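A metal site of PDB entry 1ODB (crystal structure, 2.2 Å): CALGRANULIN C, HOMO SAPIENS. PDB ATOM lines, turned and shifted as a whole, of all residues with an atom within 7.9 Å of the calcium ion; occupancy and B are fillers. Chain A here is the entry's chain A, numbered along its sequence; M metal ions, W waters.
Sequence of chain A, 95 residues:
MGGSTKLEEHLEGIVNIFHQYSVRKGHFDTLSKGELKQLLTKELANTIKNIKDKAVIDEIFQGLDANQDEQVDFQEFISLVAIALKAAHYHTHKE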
ATOM      1  N   THR A  30      -8.140   4.143 -13.072  1.00  0.00           N
ATOM      2  CA  THR A  30      -9.070   5.275 -13.050  1.00  0.00           C
ATOM      3  C   THR A  30     -10.140   5.176 -14.126  1.00  0.00           C
ATOM      4  O   THR A  30      -9.982   4.494 -15.127  1.00  0.00           O
ATOM      5  CB  THR A  30      -8.358   6.633 -13.209  1.00  0.00           C
ATOM      6  OG1 THR A  30      -7.703   6.661 -14.469  1.00  0.00           O
ATOM      7  CG2 THR A  30      -7.204   6.864 -12.174  1.00  0.00           C
ATOM      8  N   LEU A  31     -11.234   5.897 -13.888  1.00  0.00           N
ATOM      9  CA  LEU A  31     -12.358   5.960 -14.817  1.00  0.00           C
ATOM     10  C   LEU A  31     -12.256   7.215 -15.648  1.00  0.00           C
ATOM     11  O   LEU A  31     -12.272   8.324 -15.099  1.00  0.00           O
ATOM     12  CB  LEU A  31     -13.676   6.025 -14.041  1.00  0.00           C
ATOM     13  CG  LEU A  31     -13.972   4.929 -13.027  1.00  0.00           C
ATOM     14  CD1 LEU A  31     -15.091   5.337 -12.074  1.00  0.00           C
ATOM     15  CD2 LEU A  31     -14.353   3.636 -13.737  1.00  0.00           C
ATOM     16  N   PHE A  61     -19.475  13.827 -13.471  1.00  0.00           N
ATOM     17  CA  PHE A  61     -18.061  13.579 -13.711  1.00  0.00           C
ATOM     18  C   PHE A  61     -17.204  14.731 -13.147  1.00  0.00           C
ATOM     19  O   PHE A  61     -16.223  14.479 -12.458  1.00  0.00           O
ATOM     20  CB  PHE A  61     -17.792  13.417 -15.209  1.00  0.00           C
ATOM     21  CG  PHE A  61     -16.357  13.178 -15.533  1.00  0.00           C
ATOM     22  CD1 PHE A  61     -15.552  14.208 -15.986  1.00  0.00           C
ATOM     23  CD2 PHE A  61     -15.796  11.922 -15.367  1.00  0.00           C
ATOM     24  CE1 PHE A  61     -14.208  13.974 -16.296  1.00  0.00           C
ATOM     25  CE2 PHE A  61     -14.474  11.695 -15.666  1.00  0.00           C
ATOM     26  CZ  PHE A  61     -13.677  12.713 -16.129  1.00  0.00           C
ATOM     27  N   LEU A  64     -17.070  14.694  -9.401  1.00  0.00           N
ATOM     28  CA  LEU A  64     -16.240  13.606  -8.915  1.00  0.00           C
ATOM     29  C   LEU A  64     -14.728  13.859  -9.092  1.00  0.00           C
ATOM     30  O   LEU A  64     -13.906  13.497  -8.236  1.00  0.00           O
ATOM     31  CB  LEU A  64     -16.638  12.287  -9.567  1.00  0.00           C
ATOM     32  CG  LEU A  64     -17.996  11.681  -9.196  1.00  0.00           C
ATOM     33  CD1 LEU A  64     -18.136  10.294  -9.809  1.00  0.00           C
ATOM     34  CD2 LEU A  64     -18.191  11.605  -7.703  1.00  0.00           C
ATOM     35  N   ASP A  65     -14.381  14.519 -10.197  1.00  0.00           N
ATOM     36  CA  ASP A  65     -12.997  14.700 -10.594  1.00  0.00           C
ATOM     37  C   ASP A  65     -12.466  15.937  -9.920  1.00  0.00           C
ATOM     38  O   ASP A  65     -12.268  16.987 -10.551  1.00  0.00           O
ATOM     39  CB  ASP A  65     -12.895  14.804 -12.109  1.00  0.00           C
ATOM     40  CG  ASP A  65     -11.485  15.012 -12.575  1.00  0.00           C
ATOM     41  OD1 ASP A  65     -10.527  14.604 -11.861  1.00  0.00           O
ATOM     42  OD2 ASP A  65     -11.233  15.586 -13.643  1.00  0.00           O
ATOM     43  N   ALA A  66     -12.221  15.795  -8.633  1.00  0.00           N
ATOM     44  CA  ALA A  66     -12.018  16.941  -7.778  1.00  0.00           C
ATOM     45  C   ALA A  66     -10.665  17.571  -8.056  1.00  0.00           C
ATOM     46  O   ALA A  66     -10.500  18.758  -7.867  1.00  0.00           O
ATOM     47  CB  ALA A  66     -12.160  16.540  -6.311  1.00  0.00           C
ATOM     48  N   ASN A  67      -9.707  16.807  -8.573  1.00  0.00           N
ATOM     49  CA  ASN A  67      -8.411  17.386  -8.927  1.00  0.00           C
ATOM     50  C   ASN A  67      -8.232  17.743 -10.405  1.00  0.00           C
ATOM     51  O   ASN A  67      -7.131  18.113 -10.819  1.00  0.00           O
ATOM     52  CB  ASN A  67      -7.255  16.498  -8.427  1.00  0.00           C
ATOM     53  CG  ASN A  67      -7.157  15.171  -9.143  1.00  0.00           C
ATOM     54  OD1 ASN A  67      -7.887  14.888 -10.110  1.00  0.00           O
ATOM     55  ND2 ASN A  67      -6.242  14.323  -8.662  1.00  0.00           N
ATOM     56  N   GLN A  68      -9.304  17.617 -11.189  1.00  0.00           N
ATOM     57  CA  GLN A  68      -9.356  18.180 -12.550  1.00  0.00           C
ATOM     58  C   GLN A  68      -8.371  17.547 -13.512  1.00  0.00           C
ATOM     59  O   GLN A  68      -7.951  18.181 -14.459  1.00  0.00           O
ATOM     60  CB  GLN A  68      -9.066  19.683 -12.531  1.00  0.00           C
ATOM     61  CG  GLN A  68      -9.746  20.467 -11.419  1.00  0.00           C
ATOM     62  CD  GLN A  68     -11.017  21.072 -11.908  1.00  0.00           C
ATOM     63  OE1 GLN A  68     -11.945  20.321 -12.213  1.00  0.00           O
ATOM     64  NE2 GLN A  68     -11.070  22.404 -12.029  1.00  0.00           N
ATOM     65  N   ASP A  69      -7.986  16.296 -13.265  1.00  0.00           N
ATOM     66  CA  ASP A  69      -7.088  15.588 -14.181  1.00  0.00           C
ATOM     67  C   ASP A  69      -7.842  14.725 -15.212  1.00  0.00           C
ATOM     68  O   ASP A  69      -7.198  13.969 -15.942  1.00  0.00           O
ATOM     69  CB  ASP A  69      -6.051  14.775 -13.376  1.00  0.00           C
ATOM     70  CG  ASP A  69      -6.607  13.458 -12.806  1.00  0.00           C
ATOM     71  OD1 ASP A  69      -7.851  13.243 -12.709  1.00  0.00           O
ATOM     72  OD2 ASP A  69      -5.820  12.591 -12.385  1.00  0.00           O
ATOM     73  N   GLU A  70      -9.173  14.872 -15.275  1.00  0.00           N
ATOM     74  CA  GLU A  70     -10.068  14.199 -16.254  1.00  0.00           C
ATOM     75  C   GLU A  70     -10.121  12.670 -16.150  1.00  0.00           C
ATOM     76  O   GLU A  70     -10.416  11.959 -17.103  1.00  0.00           O
ATOM     77  CB  GLU A  70      -9.747  14.655 -17.677  1.00  0.00           C
ATOM     78  CG  GLU A  70     -10.021  16.155 -17.848  1.00  0.00           C
ATOM     79  CD  GLU A  70      -9.494  16.721 -19.129  1.00  0.00           C
ATOM     80  OE1 GLU A  70      -8.921  15.956 -19.952  1.00  0.00           O
ATOM     81  OE2 GLU A  70      -9.649  17.964 -19.334  1.00  0.00           O
ATOM     82  N   GLN A  71      -9.867  12.213 -14.928  1.00  0.00           N
ATOM     83  CA  GLN A  71      -9.924  10.823 -14.524  1.00  0.00           C
ATOM     84  C   GLN A  71     -10.615  10.814 -13.169  1.00  0.00           C
ATOM     85  O   GLN A  71     -10.383  11.698 -12.353  1.00  0.00           O
ATOM     86  CB  GLN A  71      -8.509  10.252 -14.349  1.00  0.00           C
ATOM     87  CG  GLN A  71      -7.700  10.156 -15.641  1.00  0.00           C
ATOM     88  CD  GLN A  71      -8.321   9.184 -16.626  1.00  0.00           C
ATOM     89  OE1 GLN A  71      -8.877   8.118 -16.241  1.00  0.00           O
ATOM     90  NE2 GLN A  71      -8.231   9.529 -17.909  1.00  0.00           N
ATOM     91  N   VAL A  72     -11.452   9.811 -12.922  1.00  0.00           N
ATOM     92  CA  VAL A  72     -11.991   9.591 -11.593  1.00  0.00           C
ATOM     93  C   VAL A  72     -11.226   8.429 -10.975  1.00  0.00           C
ATOM     94  O   VAL A  72     -11.379   7.296 -11.412  1.00  0.00           O
ATOM     95  CB  VAL A  72     -13.486   9.321 -11.613  1.00  0.00           C
ATOM     96  CG1 VAL A  72     -13.966   8.876 -10.206  1.00  0.00           C
ATOM     97  CG2 VAL A  72     -14.233  10.599 -12.104  1.00  0.00           C
ATOM     98  N   ASP A  73     -10.400   8.712  -9.979  1.00  0.00           N
ATOM     99  CA  ASP A  73      -9.661   7.658  -9.312  1.00  0.00           C
ATOM    100  C   ASP A  73     -10.493   7.000  -8.221  1.00  0.00           C
ATOM    101  O   ASP A  73     -11.698   7.303  -8.083  1.00  0.00           O
ATOM    102  CB  ASP A  73      -8.298   8.181  -8.803  1.00  0.00           C
ATOM    103  CG  ASP A  73      -8.409   9.193  -7.704  1.00  0.00           C
ATOM    104  OD1 ASP A  73      -9.263   9.074  -6.806  1.00  0.00           O
ATOM    105  OD2 ASP A  73      -7.617  10.179  -7.651  1.00  0.00           O
ATOM    106  N   PHE A  74      -9.893   6.100  -7.437  1.00  0.00           N
ATOM    107  CA  PHE A  74     -10.711   5.266  -6.577  1.00  0.00           C
ATOM    108  C   PHE A  74     -11.306   6.120  -5.418  1.00  0.00           C
ATOM    109  O   PHE A  74     -12.442   5.984  -5.060  1.00  0.00           O
ATOM    110  CB  PHE A  74      -9.948   4.056  -6.035  1.00  0.00           C
ATOM    111  CG  PHE A  74     -10.816   3.187  -5.128  1.00  0.00           C
ATOM    112  CD1 PHE A  74     -11.754   2.347  -5.654  1.00  0.00           C
ATOM    113  CD2 PHE A  74     -10.716   3.299  -3.746  1.00  0.00           C
ATOM    114  CE1 PHE A  74     -12.575   1.606  -4.822  1.00  0.00           C
ATOM    115  CE2 PHE A  74     -11.525   2.564  -2.912  1.00  0.00           C
ATOM    116  CZ  PHE A  74     -12.470   1.715  -3.464  1.00  0.00           C
ATOM    117  N   GLU A  76     -11.873   9.397  -5.490  1.00  0.00           N
ATOM    118  CA  GLU A  76     -12.918  10.225  -6.061  1.00  0.00           C
ATOM    119  C   GLU A  76     -14.185   9.383  -6.281  1.00  0.00           C
ATOM    120  O   GLU A  76     -15.271   9.886  -6.076  1.00  0.00           O
ATOM    121  CB  GLU A  76     -12.421  10.847  -7.352  1.00  0.00           C
ATOM    122  CG  GLU A  76     -11.296  11.841  -7.106  1.00  0.00           C
ATOM    123  CD  GLU A  76     -10.570  12.296  -8.358  1.00  0.00           C
ATOM    124  OE1 GLU A  76     -10.521  11.559  -9.360  1.00  0.00           O
ATOM    125  OE2 GLU A  76     -10.018  13.401  -8.350  1.00  0.00           O
HETATM  126 CA    CA M   1      -9.286  12.996 -10.860  1.00  0.00          CA
HETATM  127  O   HOH W   1      -7.545  11.535 -10.002  1.00  0.00           O
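The calcium ion is bound by O of Gln 71 (2.3 Å), OD1 of Asp 65 (2.3 Å), OD1 of Asp 69 (2.4 Å), OE1 of Glu 76 (2.4 Å), water W1 (2.4 Å), OD1 of Asn 67 (2.5 Å) and OE2 of Glu 76 (2.6 Å).
The calcium ion has seven donor atoms within binding distance.
Water W1 lies within hydrogen-bond range of the side-chain carboxylate (OD2) of Asp 73, the side-chain carboxylate (OD2) of Asp 69 and the side-chain amide nitrogen (ND2) of Asn 67.
Within 4 Å of the calcium ion: Asp 65, Asn 67, Asp 69, Gln 71 and Glu 76.
The side-chain amide oxygen of Gln 71 is in hydrogen-bond range of the side-chain hydroxyl of Thr 30 (2.6 Å).
OD1 of Asp 65 lies close to N of Gln 68, 3.3 Å away.
N of Glu 70 lies within hydrogen-bond range of OD2 of Asp 65 (2.7 Å).
OD1 of Asp 73 is in hydrogen-bond range of N of Glu 76 (2.9 Å).
N of Ala 66 sits close to OE2 of Glu 76 (3.3 Å).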
